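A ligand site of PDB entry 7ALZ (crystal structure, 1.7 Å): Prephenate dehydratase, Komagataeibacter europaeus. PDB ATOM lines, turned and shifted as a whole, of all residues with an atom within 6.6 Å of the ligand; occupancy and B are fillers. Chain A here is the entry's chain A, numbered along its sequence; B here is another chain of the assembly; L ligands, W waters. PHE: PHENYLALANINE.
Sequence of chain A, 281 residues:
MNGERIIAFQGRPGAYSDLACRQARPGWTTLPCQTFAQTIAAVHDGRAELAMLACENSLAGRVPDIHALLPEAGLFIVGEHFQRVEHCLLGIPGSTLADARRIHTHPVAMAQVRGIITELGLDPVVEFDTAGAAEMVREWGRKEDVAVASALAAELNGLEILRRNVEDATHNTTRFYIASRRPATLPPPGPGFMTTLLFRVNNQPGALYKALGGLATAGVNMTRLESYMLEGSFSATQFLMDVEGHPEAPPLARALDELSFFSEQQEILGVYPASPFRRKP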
ATOM      1  N   VAL A 201      22.813  22.463   3.938  1.00  0.00           N
ATOM      2  CA  VAL A 201      21.477  22.522   4.495  1.00  0.00           C
ATOM      3  C   VAL A 201      21.333  23.807   5.347  1.00  0.00           C
ATOM      4  O   VAL A 201      22.324  24.405   5.793  1.00  0.00           O
ATOM      5  CB  VAL A 201      21.021  21.303   5.360  1.00  0.00           C
ATOM      6  CG1 VAL A 201      21.045  19.998   4.517  1.00  0.00           C
ATOM      7  CG2 VAL A 201      21.914  21.171   6.518  1.00  0.00           C
ATOM      8  N   ASN A 202      20.081  24.237   5.531  1.00  0.00           N
ATOM      9  CA  ASN A 202      19.821  25.451   6.268  1.00  0.00           C
ATOM     10  C   ASN A 202      19.897  25.202   7.750  1.00  0.00           C
ATOM     11  O   ASN A 202      19.754  24.090   8.213  1.00  0.00           O
ATOM     12  CB  ASN A 202      18.469  25.980   5.872  1.00  0.00           C
ATOM     13  CG  ASN A 202      18.516  26.597   4.487  1.00  0.00           C
ATOM     14  OD1 ASN A 202      19.533  27.192   4.052  1.00  0.00           O
ATOM     15  ND2 ASN A 202      17.397  26.496   3.778  1.00  0.00           N
ATOM     16  N   ASN A 203      20.163  26.264   8.486  1.00  0.00           N
ATOM     17  CA  ASN A 203      20.345  26.196   9.936  1.00  0.00           C
ATOM     18  C   ASN A 203      19.007  26.247  10.679  1.00  0.00           C
ATOM     19  O   ASN A 203      18.648  27.212  11.340  1.00  0.00           O
ATOM     20  CB  ASN A 203      21.262  27.370  10.337  1.00  0.00           C
ATOM     21  CG  ASN A 203      21.573  27.454  11.825  1.00  0.00           C
ATOM     22  OD1 ASN A 203      21.985  26.434  12.469  1.00  0.00           O
ATOM     23  ND2 ASN A 203      21.386  28.677  12.384  1.00  0.00           N
ATOM     24  N   GLN A 204      18.241  25.172  10.515  1.00  0.00           N
ATOM     25  CA  GLN A 204      16.978  24.980  11.226  1.00  0.00           C
ATOM     26  C   GLN A 204      16.943  23.577  11.815  1.00  0.00           C
ATOM     27  O   GLN A 204      17.538  22.671  11.257  1.00  0.00           O
ATOM     28  CB  GLN A 204      15.772  25.134  10.257  1.00  0.00           C
ATOM     29  CG  GLN A 204      15.602  26.572   9.746  1.00  0.00           C
ATOM     30  CD  GLN A 204      15.255  27.600  10.828  1.00  0.00           C
ATOM     31  OE1 GLN A 204      14.457  27.347  11.718  1.00  0.00           O
ATOM     32  NE2 GLN A 204      15.879  28.758  10.750  1.00  0.00           N
ATOM     33  N   PRO A 205      16.233  23.354  12.947  1.00  0.00           N
ATOM     34  CA  PRO A 205      16.153  22.006  13.509  1.00  0.00           C
ATOM     35  C   PRO A 205      15.614  21.021  12.482  1.00  0.00           C
ATOM     36  O   PRO A 205      14.696  21.382  11.727  1.00  0.00           O
ATOM     37  CB  PRO A 205      15.211  22.125  14.694  1.00  0.00           C
ATOM     38  CG  PRO A 205      15.188  23.600  14.999  1.00  0.00           C
ATOM     39  CD  PRO A 205      15.574  24.366  13.794  1.00  0.00           C
ATOM     40  N   GLY A 206      16.223  19.862  12.451  1.00  0.00           N
ATOM     41  CA  GLY A 206      15.788  18.756  11.638  1.00  0.00           C
ATOM     42  C   GLY A 206      16.181  18.864  10.177  1.00  0.00           C
ATOM     43  O   GLY A 206      15.843  17.991   9.382  1.00  0.00           O
ATOM     44  N   ALA A 207      16.957  19.900   9.815  1.00  0.00           N
ATOM     45  CA  ALA A 207      17.372  20.060   8.408  1.00  0.00           C
ATOM     46  C   ALA A 207      18.257  18.938   7.903  1.00  0.00           C
ATOM     47  O   ALA A 207      18.035  18.391   6.779  1.00  0.00           O
ATOM     48  CB  ALA A 207      18.008  21.427   8.166  1.00  0.00           C
ATOM     49  N   LEU A 208      19.280  18.571   8.684  1.00  0.00           N
ATOM     50  CA  LEU A 208      20.143  17.455   8.318  1.00  0.00           C
ATOM     51  C   LEU A 208      19.344  16.138   8.291  1.00  0.00           C
ATOM     52  O   LEU A 208      19.449  15.323   7.359  1.00  0.00           O
ATOM     53  CB  LEU A 208      21.334  17.363   9.251  1.00  0.00           C
ATOM     54  CG  LEU A 208      22.266  16.195   8.988  1.00  0.00           C
ATOM     55  CD1 LEU A 208      22.901  16.109   7.589  1.00  0.00           C
ATOM     56  CD2 LEU A 208      23.310  16.135  10.090  1.00  0.00           C
ATOM     57  N   TYR A 209      18.560  15.939   9.347  1.00  0.00           N
ATOM     58  CA  TYR A 209      17.721  14.738   9.538  1.00  0.00           C
ATOM     59  C   TYR A 209      16.870  14.512   8.263  1.00  0.00           C
ATOM     60  O   TYR A 209      16.877  13.401   7.718  1.00  0.00           O
ATOM     61  CB  TYR A 209      16.851  14.964  10.732  1.00  0.00           C
ATOM     62  CG  TYR A 209      15.834  13.900  11.077  1.00  0.00           C
ATOM     63  CD1 TYR A 209      16.209  12.676  11.624  1.00  0.00           C
ATOM     64  CD2 TYR A 209      14.478  14.151  10.861  1.00  0.00           C
ATOM     65  CE1 TYR A 209      15.248  11.737  11.982  1.00  0.00           C
ATOM     66  CE2 TYR A 209      13.506  13.211  11.229  1.00  0.00           C
ATOM     67  CZ  TYR A 209      13.888  11.977  11.727  1.00  0.00           C
ATOM     68  OH  TYR A 209      12.983  11.014  12.139  1.00  0.00           O
ATOM     69  N   SER A 227      30.550  18.534   9.347  1.00  0.00           N
ATOM     70  CA  SER A 227      30.038  19.858   9.110  1.00  0.00           C
ATOM     71  C   SER A 227      31.130  20.926   9.001  1.00  0.00           C
ATOM     72  O   SER A 227      32.171  20.811   9.661  1.00  0.00           O
ATOM     73  CB  SER A 227      29.077  20.249  10.166  1.00  0.00           C
ATOM     74  OG  SER A 227      29.687  20.479  11.428  1.00  0.00           O
ATOM     75  N   ALA A 236      23.318  28.734   7.118  1.00  0.00           N
ATOM     76  CA  ALA A 236      23.413  27.394   6.580  1.00  0.00           C
ATOM     77  C   ALA A 236      24.753  26.782   6.908  1.00  0.00           C
ATOM     78  O   ALA A 236      25.689  27.498   7.333  1.00  0.00           O
ATOM     79  CB  ALA A 236      23.244  27.427   5.099  1.00  0.00           C
ATOM     80  N   THR A 237      24.823  25.464   6.753  1.00  0.00           N
ATOM     81  CA  THR A 237      26.001  24.662   7.057  1.00  0.00           C
ATOM     82  C   THR A 237      26.338  23.770   5.843  1.00  0.00           C
ATOM     83  O   THR A 237      25.432  23.137   5.240  1.00  0.00           O
ATOM     84  CB  THR A 237      25.774  23.836   8.316  1.00  0.00           C
ATOM     85  OG1 THR A 237      25.528  24.691   9.447  1.00  0.00           O
ATOM     86  CG2 THR A 237      26.877  22.804   8.594  1.00  0.00           C
ATOM     87  N   PHE A 239      28.277  20.286   4.448  1.00  0.00           N
ATOM     88  CA  PHE A 239      28.710  18.957   4.932  1.00  0.00           C
ATOM     89  C   PHE A 239      29.516  18.244   3.869  1.00  0.00           C
ATOM     90  O   PHE A 239      29.268  18.397   2.672  1.00  0.00           O
ATOM     91  CB  PHE A 239      27.482  18.048   5.237  1.00  0.00           C
ATOM     92  CG  PHE A 239      26.764  18.423   6.473  1.00  0.00           C
ATOM     93  CD1 PHE A 239      25.794  19.364   6.458  1.00  0.00           C
ATOM     94  CD2 PHE A 239      27.049  17.757   7.667  1.00  0.00           C
ATOM     95  CE1 PHE A 239      25.167  19.756   7.662  1.00  0.00           C
ATOM     96  CE2 PHE A 239      26.441  18.128   8.847  1.00  0.00           C
ATOM     97  CZ  PHE A 239      25.482  19.102   8.826  1.00  0.00           C
ATOM     98  N   LEU B 212      19.217  11.363  15.597  1.00  0.00           N
ATOM     99  CA  LEU B 212      18.919  12.772  15.373  1.00  0.00           C
ATOM    100  C   LEU B 212      17.416  13.104  15.398  1.00  0.00           C
ATOM    101  O   LEU B 212      17.054  14.260  15.485  1.00  0.00           O
ATOM    102  CB  LEU B 212      19.439  13.203  13.997  1.00  0.00           C
ATOM    103  CG  LEU B 212      20.972  13.117  13.854  1.00  0.00           C
ATOM    104  CD1 LEU B 212      21.437  13.618  12.518  1.00  0.00           C
ATOM    105  CD2 LEU B 212      21.681  13.782  14.989  1.00  0.00           C
ATOM    106  N   VAL B 220      15.318  21.268  18.435  1.00  0.00           N
ATOM    107  CA  VAL B 220      16.678  21.585  18.835  1.00  0.00           C
ATOM    108  C   VAL B 220      17.594  21.704  17.608  1.00  0.00           C
ATOM    109  O   VAL B 220      17.711  20.777  16.813  1.00  0.00           O
ATOM    110  CB  VAL B 220      17.209  20.477  19.771  1.00  0.00           C
ATOM    111  CG1 VAL B 220      18.688  20.666  20.079  1.00  0.00           C
ATOM    112  CG2 VAL B 220      16.375  20.452  21.072  1.00  0.00           C
ATOM    113  N   ASN B 221      18.250  22.864  17.503  1.00  0.00           N
ATOM    114  CA  ASN B 221      19.154  23.198  16.426  1.00  0.00           C
ATOM    115  C   ASN B 221      20.594  22.808  16.764  1.00  0.00           C
ATOM    116  O   ASN B 221      21.108  23.203  17.804  1.00  0.00           O
ATOM    117  CB  ASN B 221      19.074  24.673  16.094  1.00  0.00           C
ATOM    118  CG  ASN B 221      19.741  24.986  14.763  1.00  0.00           C
ATOM    119  OD1 ASN B 221      19.390  24.438  13.694  1.00  0.00           O
ATOM    120  ND2 ASN B 221      20.776  25.849  14.842  1.00  0.00           N
ATOM    121  N   MET B 222      21.218  22.024  15.886  1.00  0.00           N
ATOM    122  CA  MET B 222      22.623  21.668  16.006  1.00  0.00           C
ATOM    123  C   MET B 222      23.475  22.635  15.185  1.00  0.00           C
ATOM    124  O   MET B 222      23.031  23.125  14.150  1.00  0.00           O
ATOM    125  CB  MET B 222      22.880  20.237  15.478  1.00  0.00           C
ATOM    126  CG  MET B 222      22.153  19.189  16.219  1.00  0.00           C
ATOM    127  SD  MET B 222      22.521  17.405  15.469  1.00  0.00           S
ATOM    128  CE  MET B 222      21.457  17.534  13.835  1.00  0.00           C
ATOM    129  N   THR B 223      24.692  22.860  15.635  1.00  0.00           N
ATOM    130  CA  THR B 223      25.595  23.737  14.911  1.00  0.00           C
ATOM    131  C   THR B 223      26.959  23.091  14.498  1.00  0.00           C
ATOM    132  O   THR B 223      27.698  23.665  13.679  1.00  0.00           O
ATOM    133  CB  THR B 223      25.859  25.036  15.702  1.00  0.00           C
ATOM    134  OG1 THR B 223      26.456  24.776  16.980  1.00  0.00           O
ATOM    135  CG2 THR B 223      24.577  25.868  15.821  1.00  0.00           C
ATOM    136  N   ARG B 224      27.275  21.898  15.020  1.00  0.00           N
ATOM    137  CA  ARG B 224      28.444  21.144  14.561  1.00  0.00           C
ATOM    138  C   ARG B 224      28.185  19.659  14.714  1.00  0.00           C
ATOM    139  O   ARG B 224      27.544  19.211  15.675  1.00  0.00           O
ATOM    140  CB  ARG B 224      29.723  21.504  15.322  1.00  0.00           C
ATOM    141  CG  ARG B 224      30.974  20.945  14.690  1.00  0.00           C
ATOM    142  CD  ARG B 224      32.202  21.144  15.507  1.00  0.00           C
ATOM    143  NE  ARG B 224      33.370  20.547  14.862  1.00  0.00           N
ATOM    144  CZ  ARG B 224      34.565  20.397  15.416  1.00  0.00           C
ATOM    145  NH1 ARG B 224      34.785  20.781  16.665  1.00  0.00           N
ATOM    146  NH2 ARG B 224      35.545  19.823  14.689  1.00  0.00           N
ATOM    147  N   LEU B 225      28.632  18.865  13.732  1.00  0.00           N
ATOM    148  CA  LEU B 225      28.595  17.424  13.814  1.00  0.00           C
ATOM    149  C   LEU B 225      29.750  16.841  13.020  1.00  0.00           C
ATOM    150  O   LEU B 225      29.901  17.156  11.854  1.00  0.00           O
ATOM    151  CB  LEU B 225      27.274  16.909  13.255  1.00  0.00           C
ATOM    152  CG  LEU B 225      26.935  15.405  13.421  1.00  0.00           C
ATOM    153  CD1 LEU B 225      26.805  15.037  14.920  1.00  0.00           C
ATOM    154  CD2 LEU B 225      25.709  15.008  12.665  1.00  0.00           C
ATOM    155  N   MET B 241      29.270  16.521  18.651  1.00  0.00           N
ATOM    156  CA  MET B 241      28.131  17.349  18.276  1.00  0.00           C
ATOM    157  C   MET B 241      28.158  18.624  19.112  1.00  0.00           C
ATOM    158  O   MET B 241      28.381  18.552  20.320  1.00  0.00           O
ATOM    159  CB  MET B 241      26.802  16.653  18.524  1.00  0.00           C
ATOM    160  CG  MET B 241      25.611  17.508  18.187  1.00  0.00           C
ATOM    161  SD  MET B 241      23.908  16.751  18.922  1.00  0.00           S
ATOM    162  CE  MET B 241      23.954  15.451  17.771  1.00  0.00           C
ATOM    163  N   ASP B 242      27.907  19.767  18.485  1.00  0.00           N
ATOM    164  CA  ASP B 242      27.620  21.009  19.191  1.00  0.00           C
ATOM    165  C   ASP B 242      26.136  21.278  18.934  1.00  0.00           C
ATOM    166  O   ASP B 242      25.643  21.220  17.808  1.00  0.00           O
ATOM    167  CB  ASP B 242      28.371  22.246  18.631  1.00  0.00           C
ATOM    168  CG  ASP B 242      29.912  22.244  18.873  1.00  0.00           C
ATOM    169  OD1 ASP B 242      30.448  21.357  19.569  1.00  0.00           O
ATOM    170  OD2 ASP B 242      30.540  23.199  18.301  1.00  0.00           O
HETATM  171  N   PHE L   1      21.258  23.172  12.116  1.00  0.00           N
HETATM  172  CA  PHE L   1      20.755  22.102  11.225  1.00  0.00           C
HETATM  173  C   PHE L   1      20.149  20.950  12.015  1.00  0.00           C
HETATM  174  O   PHE L   1      20.173  20.965  13.282  1.00  0.00           O
HETATM  175  CB  PHE L   1      21.882  21.608  10.306  1.00  0.00           C
HETATM  176  CG  PHE L   1      23.091  21.082  11.052  1.00  0.00           C
HETATM  177  CD1 PHE L   1      23.087  19.801  11.580  1.00  0.00           C
HETATM  178  CD2 PHE L   1      24.217  21.862  11.212  1.00  0.00           C
HETATM  179  CE1 PHE L   1      24.207  19.309  12.265  1.00  0.00           C
HETATM  180  CE2 PHE L   1      25.344  21.415  11.900  1.00  0.00           C
HETATM  181  CZ  PHE L   1      25.343  20.125  12.429  1.00  0.00           C
HETATM  182  OXT PHE L   1      19.658  19.986  11.372  1.00  0.00           O
HETATM  183  O   HOH W   1      18.298  19.418  14.565  1.00  0.00           O
HETATM  184  O   HOH W   2      22.911  24.995  10.335  1.00  0.00           O
HETATM  185  O   HOH W   3      18.748  17.505  11.731  1.00  0.00           O
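The backbone NH (N) of Met 222 of chain B sits at hydrogen-bond distance from an oxygen (O) of the ligand (3.0 Å). N of the ligand lies within hydrogen-bond range of O of Met 222 of chain B (2.7 Å). The side-chain amide oxygen (OD1) of Asn 221 of chain B lies within hydrogen-bond range of a nitrogen (N) of the ligand (2.8 Å). The backbone NH (N) of Leu 208 lies within hydrogen-bond range of an oxygen (OXT) of the ligand. An oxygen (OXT) of the ligand lies within hydrogen-bond range of the backbone NH (N) of Ala 207 (3.1 Å). A nitrogen (N) of the ligand sits at hydrogen-bond distance from the side-chain amide oxygen (OD1) of Asn 203.
The side-chain amide oxygen (OD1) of Asn 221 of chain B lies close to the backbone NH (N) of Gln 204 (3.5 Å). The side-chain amide nitrogen (ND2) of Asn 221 of chain B is in hydrogen-bond range of the side-chain amide oxygen (OD1) of Asn 203 (2.7 Å). The backbone NH (N) of Thr 223 of chain B is in hydrogen-bond range of the backbone carbonyl oxygen (O) of Asp 242 of chain B (2.9 Å). The backbone carbonyl oxygen (O) of Val 201 is in hydrogen-bond range of the backbone NH (N) of Thr 237 (2.9 Å). The backbone NH (N) of Asp 242 of chain B lies within hydrogen-bond range of the backbone carbonyl oxygen (O) of Arg 224 of chain B, at 2.9 Å. The backbone NH (N) of Ser 227 sits at hydrogen-bond distance from the backbone carbonyl oxygen (O) of Leu 225 of chain B (2.9 Å).
O of Gln 204 sits close to OXT of the ligand, at 3.4 Å. Val 201 touches the ligand. Asn 202 touches the ligand (O to CA, 3.7 Å). Gly 206 touches the ligand (N to OXT, 3.6 Å). Thr 237 touches the ligand (OG1 to CD2, 3.6 Å). CZ of Phe 239 touches CE1 of the ligand, at 3.7 Å. Thr 223 of chain B touches the ligand. Arg 224 of chain B touches the ligand (C to CZ, 3.7 Å). Leu 225 of chain B touches the ligand (N to CZ, 3.8 Å). 14 residues have an atom within 4 Å of the ligand: Val 201, Asn 202, Asn 203, Gln 204, Gly 206, Ala 207, Leu 208, Thr 237, Phe 239, Asn 221 of chain B, Met 222 of chain B, Thr 223 of chain B, Arg 224 of chain B and Leu 225 of chain B. The nearest printed residue that does not touch the ligand is Pro 205 (4.2 Å).
Water W3 lies within hydrogen-bond range of an oxygen (OXT) of the ligand (2.7 Å), the backbone NH (N) of Tyr 209 (2.9 Å) and the backbone NH (N) of Leu 208 (3.3 Å). Water W1 lies within hydrogen-bond range of O of Val 220 of chain B (2.7 Å), O of the ligand (2.7 Å) and N of Gly 206 (3.0 Å). Water W2 lies within hydrogen-bond range of OD1 of Asn 203 (2.7 Å), OG1 of Thr 237 (2.8 Å) and N of the ligand (3.0 Å).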
